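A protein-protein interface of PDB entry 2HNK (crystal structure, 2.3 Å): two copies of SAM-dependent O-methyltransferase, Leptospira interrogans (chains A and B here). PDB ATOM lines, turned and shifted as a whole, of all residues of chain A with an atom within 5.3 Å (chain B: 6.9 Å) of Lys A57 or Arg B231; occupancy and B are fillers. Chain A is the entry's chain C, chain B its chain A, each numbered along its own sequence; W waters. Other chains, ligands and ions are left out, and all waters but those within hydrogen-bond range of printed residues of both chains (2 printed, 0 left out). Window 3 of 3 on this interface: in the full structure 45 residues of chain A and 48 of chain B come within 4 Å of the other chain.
The side-chain amino group (NZ) of Lys A57 is in salt-bridge range of the side-chain carboxylate (OD2) of Asp B215, 2.8 Å away.
The side-chain amino group of Lys A57 lies close to the guanidinium group of Arg B231 (3.2 Å).
The backbone NH (N) of Arg B231 lies within hydrogen-bond range of the backbone carbonyl oxygen (O) of Leu B213, at 2.9 Å.
N of Arg B229 is in hydrogen-bond range of O of Asp B215.
The side-chain carboxylate (OD2) of Asp B215 is in salt-bridge range of the guanidinium group (NH1) of Arg B231 (2.8 Å).
Among the printed residues, pairs that only touch across the chains: Ile A54 with Asp B215 (3.4 Å), Ile A54 with Arg B229 (3.7 Å) and Lys A57 with Arg B229 (3.5 Å).
Of the printed residues of chain B, Ile A54 touches Asp B215 (3.4 Å) and Arg B229 (3.7 Å).
Ile A58 touches none of the printed residues of chain B.
Of the printed residues of chain A, Asp B215 touches Ile A54 and Lys A57.
Printed residues of chain A within 4 Å of Arg B229: Ile A54 and Lys A57.
Of chain A, only Lys A57 (3.2 Å) comes within 4 Å of Arg B231.
The nearest residue of chain B that does not touch Lys A57 is Gly B174 (5.8 Å).
The nearest printed residue of chain B that does not touch Ile A54 is Val B214 (6.3 Å).
Of the 11 printed residues of chain A, 2 touch a printed residue of chain B.
Hydrophobic or aromatic side chains of chain A within 4 Å of the printed part of chain B: Ile A54.
Among the printed residues, Asp or Glu carboxylates within 4 Å of a Lys or Arg side-chain nitrogen of the other chain: Lys A57 with Asp B215 (2.8 Å).
No position is printed for both chains.
Of the 5 pairs that touch across the chains among the printed residues, none has its exchanged pair printed and touching as well.
Water W1 lies within hydrogen-bond range of the backbone carbonyl oxygen (O) of Gly B174, the guanidinium group (NE) of Arg B229 and the backbone carbonyl oxygen (O) of Lys A57.
Water W2 bridges the backbone carbonyl oxygen (O) of Lys A57 and the guanidinium group (NH2) of Arg B229.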
ATOM      1  N   LEU A  52      34.335  27.496  36.610  1.00  0.00           N
ATOM      2  CA  LEU A  52      33.773  28.531  35.731  1.00  0.00           C
ATOM      3  C   LEU A  52      33.351  27.929  34.380  1.00  0.00           C
ATOM      4  O   LEU A  52      32.290  28.247  33.856  1.00  0.00           O
ATOM      5  CB  LEU A  52      34.771  29.682  35.527  1.00  0.00           C
ATOM      6  CG  LEU A  52      35.287  30.427  36.772  1.00  0.00           C
ATOM      7  CD1 LEU A  52      36.336  31.473  36.398  1.00  0.00           C
ATOM      8  CD2 LEU A  52      34.157  31.056  37.577  1.00  0.00           C
ATOM      9  N   ASN A  53      34.195  27.048  33.849  1.00  0.00           N
ATOM     10  CA  ASN A  53      33.907  26.327  32.623  1.00  0.00           C
ATOM     11  C   ASN A  53      32.573  25.570  32.704  1.00  0.00           C
ATOM     12  O   ASN A  53      31.674  25.822  31.903  1.00  0.00           O
ATOM     13  CB  ASN A  53      35.078  25.396  32.266  1.00  0.00           C
ATOM     14  CG  ASN A  53      34.954  24.801  30.870  1.00  0.00           C
ATOM     15  OD1 ASN A  53      34.161  23.898  30.640  1.00  0.00           O
ATOM     16  ND2 ASN A  53      35.754  25.299  29.940  1.00  0.00           N
ATOM     17  N   ILE A  54      32.427  24.690  33.695  1.00  0.00           N
ATOM     18  CA  ILE A  54      31.206  23.894  33.829  1.00  0.00           C
ATOM     19  C   ILE A  54      29.961  24.763  34.056  1.00  0.00           C
ATOM     20  O   ILE A  54      28.906  24.520  33.464  1.00  0.00           O
ATOM     21  CB  ILE A  54      31.346  22.748  34.890  1.00  0.00           C
ATOM     22  CG1 ILE A  54      30.381  21.605  34.586  1.00  0.00           C
ATOM     23  CG2 ILE A  54      31.133  23.236  36.323  1.00  0.00           C
ATOM     24  CD1 ILE A  54      31.054  20.382  34.040  1.00  0.00           C
ATOM     25  N   LEU A  55      30.099  25.784  34.897  1.00  0.00           N
ATOM     26  CA  LEU A  55      29.009  26.718  35.167  1.00  0.00           C
ATOM     27  C   LEU A  55      28.543  27.452  33.913  1.00  0.00           C
ATOM     28  O   LEU A  55      27.353  27.676  33.735  1.00  0.00           O
ATOM     29  CB  LEU A  55      29.426  27.731  36.229  1.00  0.00           C
ATOM     30  CG  LEU A  55      28.896  27.678  37.669  1.00  0.00           C
ATOM     31  CD1 LEU A  55      28.372  26.322  38.136  1.00  0.00           C
ATOM     32  CD2 LEU A  55      29.969  28.222  38.630  1.00  0.00           C
ATOM     33  N   THR A  56      29.480  27.827  33.052  1.00  0.00           N
ATOM     34  CA  THR A  56      29.134  28.493  31.789  1.00  0.00           C
ATOM     35  C   THR A  56      28.272  27.573  30.920  1.00  0.00           C
ATOM     36  O   THR A  56      27.254  27.994  30.388  1.00  0.00           O
ATOM     37  CB  THR A  56      30.398  28.946  31.032  1.00  0.00           C
ATOM     38  OG1 THR A  56      31.106  29.886  31.845  1.00  0.00           O
ATOM     39  CG2 THR A  56      30.050  29.597  29.690  1.00  0.00           C
ATOM     40  N   LYS A  57      28.683  26.314  30.821  1.00  0.00           N
ATOM     41  CA  LYS A  57      27.957  25.300  30.060  1.00  0.00           C
ATOM     42  C   LYS A  57      26.584  24.964  30.651  1.00  0.00           C
ATOM     43  O   LYS A  57      25.596  24.911  29.929  1.00  0.00           O
ATOM     44  CB  LYS A  57      28.811  24.033  29.927  1.00  0.00           C
ATOM     45  CG  LYS A  57      30.158  24.281  29.308  1.00  0.00           C
ATOM     46  CD  LYS A  57      30.846  22.988  28.927  1.00  0.00           C
ATOM     47  CE  LYS A  57      32.046  23.271  28.041  1.00  0.00           C
ATOM     48  NZ  LYS A  57      32.668  22.014  27.546  1.00  0.00           N
ATOM     49  N   ILE A  58      26.533  24.753  31.962  1.00  0.00           N
ATOM     50  CA  ILE A  58      25.295  24.431  32.669  1.00  0.00           C
ATOM     51  C   ILE A  58      24.276  25.558  32.487  1.00  0.00           C
ATOM     52  O   ILE A  58      23.108  25.302  32.200  1.00  0.00           O
ATOM     53  CB  ILE A  58      25.568  24.163  34.196  1.00  0.00           C
ATOM     54  CG1 ILE A  58      26.349  22.861  34.392  1.00  0.00           C
ATOM     55  CG2 ILE A  58      24.282  24.137  35.006  1.00  0.00           C
ATOM     56  CD1 ILE A  58      26.932  22.693  35.813  1.00  0.00           C
ATOM     57  N   SER A  59      24.734  26.799  32.638  1.00  0.00           N
ATOM     58  CA  SER A  59      23.869  27.971  32.544  1.00  0.00           C
ATOM     59  C   SER A  59      23.333  28.267  31.137  1.00  0.00           C
ATOM     60  O   SER A  59      22.353  29.001  30.987  1.00  0.00           O
ATOM     61  CB  SER A  59      24.604  29.203  33.077  1.00  0.00           C
ATOM     62  OG  SER A  59      25.641  29.597  32.201  1.00  0.00           O
ATOM     63  N   GLY A  60      23.978  27.716  30.114  1.00  0.00           N
ATOM     64  CA  GLY A  60      23.614  27.996  28.718  1.00  0.00           C
ATOM     65  C   GLY A  60      23.982  29.399  28.254  1.00  0.00           C
ATOM     66  O   GLY A  60      23.541  29.835  27.192  1.00  0.00           O
ATOM     67  N   SER A  80      36.556  29.324  26.013  1.00  0.00           N
ATOM     68  CA  SER A  80      36.509  27.943  25.531  1.00  0.00           C
ATOM     69  C   SER A  80      35.253  27.175  25.944  1.00  0.00           C
ATOM     70  O   SER A  80      34.884  26.213  25.277  1.00  0.00           O
ATOM     71  CB  SER A  80      37.770  27.153  25.894  1.00  0.00           C
ATOM     72  OG  SER A  80      38.290  27.540  27.140  1.00  0.00           O
ATOM     73  N   ALA A  81      34.601  27.596  27.029  1.00  0.00           N
ATOM     74  CA  ALA A  81      33.359  26.952  27.479  1.00  0.00           C
ATOM     75  C   ALA A  81      32.144  27.393  26.671  1.00  0.00           C
ATOM     76  O   ALA A  81      31.218  26.608  26.490  1.00  0.00           O
ATOM     77  CB  ALA A  81      33.115  27.201  28.958  1.00  0.00           C
ATOM     78  N   LYS B 172      19.852  13.512  29.395  1.00  0.00           N
ATOM     79  CA  LYS B 172      19.861  14.190  28.104  1.00  0.00           C
ATOM     80  C   LYS B 172      21.272  14.712  27.825  1.00  0.00           C
ATOM     81  O   LYS B 172      22.054  14.904  28.764  1.00  0.00           O
ATOM     82  CB  LYS B 172      18.901  15.376  28.116  1.00  0.00           C
ATOM     83  CG  LYS B 172      17.425  15.046  28.252  1.00  0.00           C
ATOM     84  CD  LYS B 172      16.662  16.357  28.201  1.00  0.00           C
ATOM     85  CE  LYS B 172      15.207  16.202  28.569  1.00  0.00           C
ATOM     86  NZ  LYS B 172      14.611  17.564  28.743  1.00  0.00           N
ATOM     87  N   PRO B 173      21.621  14.925  26.537  1.00  0.00           N
ATOM     88  CA  PRO B 173      22.861  15.650  26.277  1.00  0.00           C
ATOM     89  C   PRO B 173      22.774  17.039  26.913  1.00  0.00           C
ATOM     90  O   PRO B 173      21.727  17.683  26.850  1.00  0.00           O
ATOM     91  CB  PRO B 173      22.903  15.750  24.749  1.00  0.00           C
ATOM     92  CG  PRO B 173      22.011  14.633  24.258  1.00  0.00           C
ATOM     93  CD  PRO B 173      20.938  14.513  25.292  1.00  0.00           C
ATOM     94  N   GLY B 174      23.852  17.482  27.545  1.00  0.00           N
ATOM     95  CA  GLY B 174      23.834  18.755  28.258  1.00  0.00           C
ATOM     96  C   GLY B 174      23.313  18.637  29.679  1.00  0.00           C
ATOM     97  O   GLY B 174      23.360  19.602  30.426  1.00  0.00           O
ATOM     98  N   GLY B 175      22.814  17.452  30.045  1.00  0.00           N
ATOM     99  CA  GLY B 175      22.293  17.181  31.389  1.00  0.00           C
ATOM    100  C   GLY B 175      23.383  17.107  32.449  1.00  0.00           C
ATOM    101  O   GLY B 175      24.560  16.916  32.140  1.00  0.00           O
ATOM    102  N   ASP B 211      36.504  10.154  31.047  1.00  0.00           N
ATOM    103  CA  ASP B 211      35.386  10.068  30.117  1.00  0.00           C
ATOM    104  C   ASP B 211      35.248  11.328  29.274  1.00  0.00           C
ATOM    105  O   ASP B 211      34.792  12.359  29.757  1.00  0.00           O
ATOM    106  CB  ASP B 211      34.081   9.775  30.869  1.00  0.00           C
ATOM    107  CG  ASP B 211      32.950   9.351  29.946  1.00  0.00           C
ATOM    108  OD1 ASP B 211      33.100   9.409  28.707  1.00  0.00           O
ATOM    109  OD2 ASP B 211      31.893   8.966  30.469  1.00  0.00           O
ATOM    110  N   SER B 212      35.623  11.228  28.001  1.00  0.00           N
ATOM    111  CA  SER B 212      35.519  12.357  27.072  1.00  0.00           C
ATOM    112  C   SER B 212      34.074  12.713  26.710  1.00  0.00           C
ATOM    113  O   SER B 212      33.835  13.676  25.997  1.00  0.00           O
ATOM    114  CB  SER B 212      36.346  12.104  25.808  1.00  0.00           C
ATOM    115  OG  SER B 212      35.929  10.914  25.168  1.00  0.00           O
ATOM    116  N   LEU B 213      33.111  11.948  27.209  1.00  0.00           N
ATOM    117  CA  LEU B 213      31.710  12.276  26.974  1.00  0.00           C
ATOM    118  C   LEU B 213      31.151  13.248  28.017  1.00  0.00           C
ATOM    119  O   LEU B 213      30.016  13.706  27.904  1.00  0.00           O
ATOM    120  CB  LEU B 213      30.858  11.005  26.875  1.00  0.00           C
ATOM    121  CG  LEU B 213      31.230   9.997  25.770  1.00  0.00           C
ATOM    122  CD1 LEU B 213      30.397   8.730  25.910  1.00  0.00           C
ATOM    123  CD2 LEU B 213      31.091  10.601  24.364  1.00  0.00           C
ATOM    124  N   VAL B 214      31.964  13.570  29.020  1.00  0.00           N
ATOM    125  CA  VAL B 214      31.569  14.480  30.089  1.00  0.00           C
ATOM    126  C   VAL B 214      32.651  15.513  30.353  1.00  0.00           C
ATOM    127  O   VAL B 214      33.794  15.327  29.942  1.00  0.00           O
ATOM    128  CB  VAL B 214      31.237  13.729  31.423  1.00  0.00           C
ATOM    129  CG1 VAL B 214      30.204  12.625  31.196  1.00  0.00           C
ATOM    130  CG2 VAL B 214      32.492  13.191  32.107  1.00  0.00           C
ATOM    131  N   ASP B 215      32.265  16.606  31.013  1.00  0.00           N
ATOM    132  CA  ASP B 215      33.192  17.470  31.725  1.00  0.00           C
ATOM    133  C   ASP B 215      32.897  17.361  33.228  1.00  0.00           C
ATOM    134  O   ASP B 215      31.757  17.097  33.620  1.00  0.00           O
ATOM    135  CB  ASP B 215      33.036  18.930  31.273  1.00  0.00           C
ATOM    136  CG  ASP B 215      33.369  19.129  29.802  1.00  0.00           C
ATOM    137  OD1 ASP B 215      34.516  18.796  29.414  1.00  0.00           O
ATOM    138  OD2 ASP B 215      32.492  19.622  29.039  1.00  0.00           O
ATOM    139  N   ARG B 229      28.864  17.051  33.734  1.00  0.00           N
ATOM    140  CA  ARG B 229      27.926  17.458  32.697  1.00  0.00           C
ATOM    141  C   ARG B 229      28.110  16.611  31.450  1.00  0.00           C
ATOM    142  O   ARG B 229      29.210  16.529  30.900  1.00  0.00           O
ATOM    143  CB  ARG B 229      28.072  18.951  32.357  1.00  0.00           C
ATOM    144  CG  ARG B 229      27.096  19.437  31.298  1.00  0.00           C
ATOM    145  CD  ARG B 229      27.428  20.849  30.820  1.00  0.00           C
ATOM    146  NE  ARG B 229      26.680  21.239  29.616  1.00  0.00           N
ATOM    147  CZ  ARG B 229      27.113  21.043  28.371  1.00  0.00           C
ATOM    148  NH1 ARG B 229      28.282  20.457  28.141  1.00  0.00           N
ATOM    149  NH2 ARG B 229      26.372  21.429  27.344  1.00  0.00           N
ATOM    150  N   LYS B 230      27.023  15.980  31.022  1.00  0.00           N
ATOM    151  CA  LYS B 230      27.025  15.161  29.823  1.00  0.00           C
ATOM    152  C   LYS B 230      27.113  16.084  28.602  1.00  0.00           C
ATOM    153  O   LYS B 230      26.244  16.915  28.387  1.00  0.00           O
ATOM    154  CB  LYS B 230      25.780  14.268  29.781  1.00  0.00           C
ATOM    155  CG  LYS B 230      25.720  13.331  28.579  1.00  0.00           C
ATOM    156  CD  LYS B 230      24.446  12.488  28.590  1.00  0.00           C
ATOM    157  CE  LYS B 230      24.261  11.735  27.287  1.00  0.00           C
ATOM    158  NZ  LYS B 230      23.124  10.784  27.388  1.00  0.00           N
ATOM    159  N   ARG B 231      28.183  15.946  27.828  1.00  0.00           N
ATOM    160  CA  ARG B 231      28.434  16.831  26.695  1.00  0.00           C
ATOM    161  C   ARG B 231      27.425  16.673  25.561  1.00  0.00           C
ATOM    162  O   ARG B 231      26.852  15.597  25.362  1.00  0.00           O
ATOM    163  CB  ARG B 231      29.857  16.635  26.176  1.00  0.00           C
ATOM    164  CG  ARG B 231      30.895  17.198  27.109  1.00  0.00           C
ATOM    165  CD  ARG B 231      32.271  16.665  26.817  1.00  0.00           C
ATOM    166  NE  ARG B 231      32.792  17.185  25.559  1.00  0.00           N
ATOM    167  CZ  ARG B 231      33.415  18.354  25.425  1.00  0.00           C
ATOM    168  NH1 ARG B 231      33.597  19.146  26.478  1.00  0.00           N
ATOM    169  NH2 ARG B 231      33.849  18.733  24.229  1.00  0.00           N
ATOM    170  N   LEU B 232      27.204  17.760  24.831  1.00  0.00           N
ATOM    171  CA  LEU B 232      26.346  17.735  23.644  1.00  0.00           C
ATOM    172  C   LEU B 232      26.998  16.883  22.566  1.00  0.00           C
ATOM    173  O   LEU B 232      28.223  16.762  22.502  1.00  0.00           O
ATOM    174  CB  LEU B 232      26.063  19.152  23.133  1.00  0.00           C
ATOM    175  CG  LEU B 232      25.402  20.101  24.135  1.00  0.00           C
ATOM    176  CD1 LEU B 232      25.434  21.533  23.630  1.00  0.00           C
ATOM    177  CD2 LEU B 232      23.970  19.682  24.462  1.00  0.00           C
ATOM    178  N   GLU B 233      26.173  16.273  21.728  1.00  0.00           N
ATOM    179  CA  GLU B 233      26.680  15.318  20.748  1.00  0.00           C
ATOM    180  C   GLU B 233      26.910  15.926  19.358  1.00  0.00           C
ATOM    181  O   GLU B 233      26.115  15.735  18.432  1.00  0.00           O
ATOM    182  CB  GLU B 233      25.802  14.056  20.722  1.00  0.00           C
ATOM    183  CG  GLU B 233      26.153  13.078  21.854  1.00  0.00           C
ATOM    184  CD  GLU B 233      24.961  12.277  22.382  1.00  0.00           C
ATOM    185  OE1 GLU B 233      23.905  12.238  21.705  1.00  0.00           O
ATOM    186  OE2 GLU B 233      25.091  11.685  23.482  1.00  0.00           O
ATOM    187  N   HIS B 234      27.994  16.691  19.243  1.00  0.00           N
ATOM    188  CA  HIS B 234      28.574  17.051  17.946  1.00  0.00           C
ATOM    189  C   HIS B 234      30.010  16.541  17.874  1.00  0.00           C
ATOM    190  O   HIS B 234      30.403  15.655  18.649  1.00  0.00           O
ATOM    191  CB  HIS B 234      28.519  18.563  17.676  1.00  0.00           C
ATOM    192  CG  HIS B 234      28.650  19.415  18.902  1.00  0.00           C
ATOM    193  ND1 HIS B 234      27.731  20.393  19.229  1.00  0.00           N
ATOM    194  CD2 HIS B 234      29.588  19.438  19.881  1.00  0.00           C
ATOM    195  CE1 HIS B 234      28.099  20.983  20.353  1.00  0.00           C
ATOM    196  NE2 HIS B 234      29.220  20.420  20.771  1.00  0.00           N
HETATM  197  O   HOH W   1      24.113  22.036  29.711  1.00  0.00           O
HETATM  198  O   HOH W   2      25.029  24.355  27.376  1.00  0.00           O
